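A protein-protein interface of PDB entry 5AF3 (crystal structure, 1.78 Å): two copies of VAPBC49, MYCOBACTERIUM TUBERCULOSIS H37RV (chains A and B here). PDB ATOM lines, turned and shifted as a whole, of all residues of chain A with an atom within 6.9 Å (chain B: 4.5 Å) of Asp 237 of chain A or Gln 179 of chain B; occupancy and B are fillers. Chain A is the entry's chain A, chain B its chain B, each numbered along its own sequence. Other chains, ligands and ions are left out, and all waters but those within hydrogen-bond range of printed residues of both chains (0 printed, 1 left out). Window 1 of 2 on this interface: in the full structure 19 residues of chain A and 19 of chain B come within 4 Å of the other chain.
The backbone carbonyl oxygen of Tyr 26 of chain B lies close to the side-chain amide oxygen of Gln 179 of chain B (2.7 Å).
His 159 of chain B touches Arg 233 of chain A. Leu 236 of chain A touches Tyr 160 of chain B. Asp 237 of chain A touches Pro 178 of chain B (OD2 to CB, 3.1 Å). Gln 179 of chain B touches Asp 237 of chain A (CB to O, 2.9 Å).
2 positions are printed for both chains. Of the 6 pairs that touch across the chains among the printed residues, none has its exchanged pair printed and touching as well.
Asp 237 of chain A touches four residues of chain B. Gln 179 of chain B touches just one residue of chain A: Asp 237 (2.9 Å). Of the printed residues of chain A, Pro 178 of chain B touches Asp 237. Of the printed residues of chain A, His 159 of chain B touches Arg 233 and Asp 237. Printed residues of chain B within 4 Å of Arg 233 of chain A: His 159. Of the printed residues of chain A, Tyr 160 of chain B touches Leu 236 (3.5 Å) and Asp 237 (2.3 Å). Gly 181 of chain B touches none of the printed residues of chain A. The nearest printed residue of chain B that does not touch Asp 237 of chain A is Tyr 180 of chain B (5.4 Å). The nearest residue of chain A that does not touch Gln 179 of chain B is Gln 179 of chain A (5.0 Å).
Hydrophobic or aromatic side chains of chain A that line the printed part of chain B: Leu 236. Of the 10 printed residues of chain B, 4 touch a printed residue of chain A. Printed residues of chain B that touch a printed residue of chain A: His 159, Tyr 160, Pro 178 and Gln 179. Among the printed residues, 6 pairs touch across the chains. Among the printed residues, no Asp or Glu carboxylate lies within 4 Å of a Lys or Arg side-chain nitrogen of the other chain.
A ring nitrogen (NE2) of His 159 of chain B lies within hydrogen-bond range of the side-chain carboxylate of Asp 237 of chain A. The side-chain hydroxyl (OH) of Tyr 160 of chain B sits close to the side-chain carboxylate (OD1) of Asp 237 of chain A, 2.3 Å away.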
ATOM      1  N   GLN A 179      11.111  27.305  16.394  1.00  0.00           N
ATOM      2  CA  GLN A 179      10.653  26.852  15.063  1.00  0.00           C
ATOM      3  C   GLN A 179      11.813  26.834  14.063  1.00  0.00           C
ATOM      4  O   GLN A 179      11.728  26.139  13.044  1.00  0.00           O
ATOM      5  CB  GLN A 179       9.489  27.664  14.507  1.00  0.00           C
ATOM      6  CG  GLN A 179       9.779  29.123  14.084  1.00  0.00           C
ATOM      7  CD  GLN A 179       9.455  30.146  15.175  1.00  0.00           C
ATOM      8  OE1 GLN A 179       8.971  31.249  14.869  1.00  0.00           O
ATOM      9  NE2 GLN A 179       9.706  29.790  16.430  1.00  0.00           N
ATOM     10  N   TYR A 180      12.897  27.564  14.376  1.00  0.00           N
ATOM     11  CA  TYR A 180      14.101  27.555  13.522  1.00  0.00           C
ATOM     12  C   TYR A 180      15.110  26.474  13.923  1.00  0.00           C
ATOM     13  O   TYR A 180      16.159  26.333  13.296  1.00  0.00           O
ATOM     14  CB  TYR A 180      14.788  28.916  13.522  1.00  0.00           C
ATOM     15  CG  TYR A 180      14.045  30.026  12.874  1.00  0.00           C
ATOM     16  CD1 TYR A 180      13.133  30.796  13.611  1.00  0.00           C
ATOM     17  CD2 TYR A 180      14.247  30.344  11.519  1.00  0.00           C
ATOM     18  CE1 TYR A 180      12.475  31.837  13.040  1.00  0.00           C
ATOM     19  CE2 TYR A 180      13.594  31.397  10.939  1.00  0.00           C
ATOM     20  CZ  TYR A 180      12.704  32.143  11.699  1.00  0.00           C
ATOM     21  OH  TYR A 180      12.032  33.201  11.149  1.00  0.00           O
ATOM     22  N   LEU A 232      21.178  26.576   7.757  1.00  0.00           N
ATOM     23  CA  LEU A 232      20.433  27.241   6.689  1.00  0.00           C
ATOM     24  C   LEU A 232      19.160  26.480   6.338  1.00  0.00           C
ATOM     25  O   LEU A 232      18.125  27.100   6.128  1.00  0.00           O
ATOM     26  CB  LEU A 232      21.254  27.395   5.412  1.00  0.00           C
ATOM     27  CG  LEU A 232      22.229  28.521   5.254  1.00  0.00           C
ATOM     28  CD1 LEU A 232      22.891  28.385   3.867  1.00  0.00           C
ATOM     29  CD2 LEU A 232      21.576  29.941   5.479  1.00  0.00           C
ATOM     30  N   ARG A 233      19.258  25.148   6.204  1.00  0.00           N
ATOM     31  CA  ARG A 233      18.067  24.348   5.884  1.00  0.00           C
ATOM     32  C   ARG A 233      17.008  24.539   6.969  1.00  0.00           C
ATOM     33  O   ARG A 233      15.807  24.735   6.665  1.00  0.00           O
ATOM     34  CB  ARG A 233      18.416  22.866   5.707  1.00  0.00           C
ATOM     35  CG  ARG A 233      19.109  22.549   4.380  1.00  0.00           C
ATOM     36  CD  ARG A 233      19.803  21.152   4.402  1.00  0.00           C
ATOM     37  NE  ARG A 233      20.816  21.110   3.362  1.00  0.00           N
ATOM     38  CZ  ARG A 233      22.129  21.012   3.551  1.00  0.00           C
ATOM     39  NH1 ARG A 233      22.664  20.859   4.764  1.00  0.00           N
ATOM     40  NH2 ARG A 233      22.916  21.027   2.491  1.00  0.00           N
ATOM     41  N   ASP A 234      17.458  24.507   8.232  1.00  0.00           N
ATOM     42  CA  ASP A 234      16.580  24.780   9.381  1.00  0.00           C
ATOM     43  C   ASP A 234      15.906  26.146   9.305  1.00  0.00           C
ATOM     44  O   ASP A 234      14.701  26.282   9.546  1.00  0.00           O
ATOM     45  CB  ASP A 234      17.385  24.652  10.686  1.00  0.00           C
ATOM     46  CG  ASP A 234      17.757  23.230  10.999  1.00  0.00           C
ATOM     47  OD1 ASP A 234      17.254  22.308  10.309  1.00  0.00           O
ATOM     48  OD2 ASP A 234      18.567  23.032  11.926  1.00  0.00           O
ATOM     49  N   ALA A 235      16.659  27.177   8.959  1.00  0.00           N
ATOM     50  CA  ALA A 235      16.058  28.507   8.817  1.00  0.00           C
ATOM     51  C   ALA A 235      15.024  28.536   7.696  1.00  0.00           C
ATOM     52  O   ALA A 235      13.962  29.096   7.856  1.00  0.00           O
ATOM     53  CB  ALA A 235      17.130  29.596   8.585  1.00  0.00           C
ATOM     54  N   LEU A 236      15.347  27.930   6.554  1.00  0.00           N
ATOM     55  CA  LEU A 236      14.500  28.002   5.408  1.00  0.00           C
ATOM     56  C   LEU A 236      13.123  27.426   5.685  1.00  0.00           C
ATOM     57  O   LEU A 236      12.118  27.969   5.237  1.00  0.00           O
ATOM     58  CB  LEU A 236      15.187  27.234   4.267  1.00  0.00           C
ATOM     59  CG  LEU A 236      14.865  27.472   2.815  1.00  0.00           C
ATOM     60  CD1 LEU A 236      15.052  28.943   2.407  1.00  0.00           C
ATOM     61  CD2 LEU A 236      15.793  26.498   2.004  1.00  0.00           C
ATOM     62  N   ASP A 237      13.120  26.313   6.419  1.00  0.00           N
ATOM     63  CA  ASP A 237      11.976  25.413   6.675  1.00  0.00           C
ATOM     64  C   ASP A 237      11.217  25.716   7.956  1.00  0.00           C
ATOM     65  O   ASP A 237      10.292  24.988   8.316  1.00  0.00           O
ATOM     66  CB  ASP A 237      12.476  23.940   6.754  1.00  0.00           C
ATOM     67  CG  ASP A 237      13.146  23.442   5.453  1.00  0.00           C
ATOM     68  OD1 ASP A 237      12.746  23.885   4.371  1.00  0.00           O
ATOM     69  OD2 ASP A 237      14.068  22.594   5.523  1.00  0.00           O
ATOM     70  N   ALA A 238      11.623  26.756   8.677  1.00  0.00           N
ATOM     71  CA  ALA A 238      10.878  27.192   9.875  1.00  0.00           C
ATOM     72  C   ALA A 238       9.420  27.655   9.606  1.00  0.00           C
ATOM     73  O   ALA A 238       9.205  28.556   8.802  1.00  0.00           O
ATOM     74  CB  ALA A 238      11.684  28.288  10.638  1.00  0.00           C
ATOM     75  N   ARG B  25      -1.803  23.633   5.312  1.00  0.00           N
ATOM     76  CA  ARG B  25      -1.054  23.482   6.569  1.00  0.00           C
ATOM     77  C   ARG B  25       0.197  22.600   6.415  1.00  0.00           C
ATOM     78  O   ARG B  25       1.313  22.996   6.771  1.00  0.00           O
ATOM     79  CB  ARG B  25      -1.989  22.925   7.648  1.00  0.00           C
ATOM     80  CG  ARG B  25      -1.535  23.281   9.031  1.00  0.00           C
ATOM     81  CD  ARG B  25      -2.694  23.256   9.989  1.00  0.00           C
ATOM     82  NE  ARG B  25      -2.777  24.496  10.760  1.00  0.00           N
ATOM     83  CZ  ARG B  25      -2.127  24.756  11.898  1.00  0.00           C
ATOM     84  NH1 ARG B  25      -1.297  23.865  12.453  1.00  0.00           N
ATOM     85  NH2 ARG B  25      -2.313  25.932  12.491  1.00  0.00           N
ATOM     86  N   TYR B  26       0.014  21.420   5.829  1.00  0.00           N
ATOM     87  CA  TYR B  26       1.128  20.473   5.682  1.00  0.00           C
ATOM     88  C   TYR B  26       2.253  20.972   4.764  1.00  0.00           C
ATOM     89  O   TYR B  26       3.409  20.758   5.049  1.00  0.00           O
ATOM     90  CB  TYR B  26       0.627  19.097   5.211  1.00  0.00           C
ATOM     91  CG  TYR B  26      -0.586  18.510   5.929  1.00  0.00           C
ATOM     92  CD1 TYR B  26      -0.892  18.816   7.279  1.00  0.00           C
ATOM     93  CD2 TYR B  26      -1.437  17.634   5.258  1.00  0.00           C
ATOM     94  CE1 TYR B  26      -2.017  18.242   7.921  1.00  0.00           C
ATOM     95  CE2 TYR B  26      -2.555  17.076   5.899  1.00  0.00           C
ATOM     96  CZ  TYR B  26      -2.826  17.388   7.223  1.00  0.00           C
ATOM     97  OH  TYR B  26      -3.934  16.808   7.819  1.00  0.00           O
ATOM     98  N   VAL B  28       2.688  24.264   3.904  1.00  0.00           N
ATOM     99  CA  VAL B  28       3.013  25.682   4.235  1.00  0.00           C
ATOM    100  C   VAL B  28       2.895  26.535   2.959  1.00  0.00           C
ATOM    101  O   VAL B  28       3.901  27.065   2.420  1.00  0.00           O
ATOM    102  CB  VAL B  28       4.411  25.874   4.890  1.00  0.00           C
ATOM    103  CG1 VAL B  28       4.469  27.251   5.607  1.00  0.00           C
ATOM    104  CG2 VAL B  28       4.720  24.766   5.887  1.00  0.00           C
ATOM    105  N   HIS B 159      16.832  20.751  -2.438  1.00  0.00           N
ATOM    106  CA  HIS B 159      16.525  20.477  -1.007  1.00  0.00           C
ATOM    107  C   HIS B 159      15.134  19.868  -0.818  1.00  0.00           C
ATOM    108  O   HIS B 159      14.947  18.886  -0.049  1.00  0.00           O
ATOM    109  CB  HIS B 159      16.666  21.766  -0.174  1.00  0.00           C
ATOM    110  CG  HIS B 159      16.173  21.665   1.244  1.00  0.00           C
ATOM    111  ND1 HIS B 159      16.611  20.698   2.126  1.00  0.00           N
ATOM    112  CD2 HIS B 159      15.297  22.432   1.937  1.00  0.00           C
ATOM    113  CE1 HIS B 159      16.026  20.867   3.298  1.00  0.00           C
ATOM    114  NE2 HIS B 159      15.233  21.921   3.214  1.00  0.00           N
ATOM    115  N   TYR B 160      14.151  20.458  -1.476  1.00  0.00           N
ATOM    116  CA  TYR B 160      12.802  19.946  -1.345  1.00  0.00           C
ATOM    117  C   TYR B 160      12.538  18.697  -2.187  1.00  0.00           C
ATOM    118  O   TYR B 160      11.798  17.814  -1.763  1.00  0.00           O
ATOM    119  CB  TYR B 160      11.768  21.015  -1.617  1.00  0.00           C
ATOM    120  CG  TYR B 160      11.895  22.082  -0.567  1.00  0.00           C
ATOM    121  CD1 TYR B 160      11.274  21.933   0.666  1.00  0.00           C
ATOM    122  CD2 TYR B 160      12.693  23.198  -0.795  1.00  0.00           C
ATOM    123  CE1 TYR B 160      11.446  22.889   1.674  1.00  0.00           C
ATOM    124  CE2 TYR B 160      12.872  24.176   0.182  1.00  0.00           C
ATOM    125  CZ  TYR B 160      12.257  24.020   1.403  1.00  0.00           C
ATOM    126  OH  TYR B 160      12.438  24.984   2.362  1.00  0.00           O
ATOM    127  N   LEU B 177       8.499  16.161   5.483  1.00  0.00           N
ATOM    128  CA  LEU B 177       8.206  17.613   5.680  1.00  0.00           C
ATOM    129  C   LEU B 177       9.353  18.230   6.518  1.00  0.00           C
ATOM    130  O   LEU B 177       9.504  17.950   7.710  1.00  0.00           O
ATOM    131  CB  LEU B 177       6.801  17.794   6.287  1.00  0.00           C
ATOM    132  CG  LEU B 177       5.674  17.081   5.533  1.00  0.00           C
ATOM    133  CD1 LEU B 177       4.434  17.232   6.297  1.00  0.00           C
ATOM    134  CD2 LEU B 177       5.494  17.626   4.081  1.00  0.00           C
ATOM    135  N   PRO B 178      10.256  18.991   5.860  1.00  0.00           N
ATOM    136  CA  PRO B 178      11.481  19.393   6.545  1.00  0.00           C
ATOM    137  C   PRO B 178      11.219  20.435   7.650  1.00  0.00           C
ATOM    138  O   PRO B 178      12.086  20.636   8.497  1.00  0.00           O
ATOM    139  CB  PRO B 178      12.354  19.965   5.418  1.00  0.00           C
ATOM    140  CG  PRO B 178      11.403  20.408   4.389  1.00  0.00           C
ATOM    141  CD  PRO B 178      10.209  19.478   4.466  1.00  0.00           C
ATOM    142  N   GLN B 179      10.030  21.007   7.668  1.00  0.00           N
ATOM    143  CA  GLN B 179       9.676  21.976   8.720  1.00  0.00           C
ATOM    144  C   GLN B 179       9.602  21.317  10.080  1.00  0.00           C
ATOM    145  O   GLN B 179       9.698  22.010  11.101  1.00  0.00           O
ATOM    146  CB  GLN B 179       8.389  22.744   8.440  1.00  0.00           C
ATOM    147  CG  GLN B 179       7.051  21.987   8.445  1.00  0.00           C
ATOM    148  CD  GLN B 179       6.668  21.437   7.071  1.00  0.00           C
ATOM    149  OE1 GLN B 179       5.482  21.376   6.736  1.00  0.00           O
ATOM    150  NE2 GLN B 179       7.661  21.069   6.273  1.00  0.00           N
ATOM    151  N   TYR B 180       9.443  19.987  10.082  1.00  0.00           N
ATOM    152  CA  TYR B 180       9.429  19.212  11.337  1.00  0.00           C
ATOM    153  C   TYR B 180      10.832  18.748  11.771  1.00  0.00           C
ATOM    154  O   TYR B 180      10.995  18.125  12.813  1.00  0.00           O
ATOM    155  CB  TYR B 180       8.490  18.014  11.195  1.00  0.00           C
ATOM    156  CG  TYR B 180       7.040  18.323  11.109  1.00  0.00           C
ATOM    157  CD1 TYR B 180       6.418  18.529   9.866  1.00  0.00           C
ATOM    158  CD2 TYR B 180       6.249  18.380  12.265  1.00  0.00           C
ATOM    159  CE1 TYR B 180       5.062  18.755   9.786  1.00  0.00           C
ATOM    160  CE2 TYR B 180       4.916  18.623  12.197  1.00  0.00           C
ATOM    161  CZ  TYR B 180       4.316  18.816  10.963  1.00  0.00           C
ATOM    162  OH  TYR B 180       2.983  19.054  10.869  1.00  0.00           O
ATOM    163  N   GLY B 181      11.845  19.021  10.957  1.00  0.00           N
ATOM    164  CA  GLY B 181      13.224  18.788  11.341  1.00  0.00           C
ATOM    165  C   GLY B 181      13.530  17.322  11.627  1.00  0.00           C
ATOM    166  O   GLY B 181      13.044  16.438  10.928  1.00  0.00           O
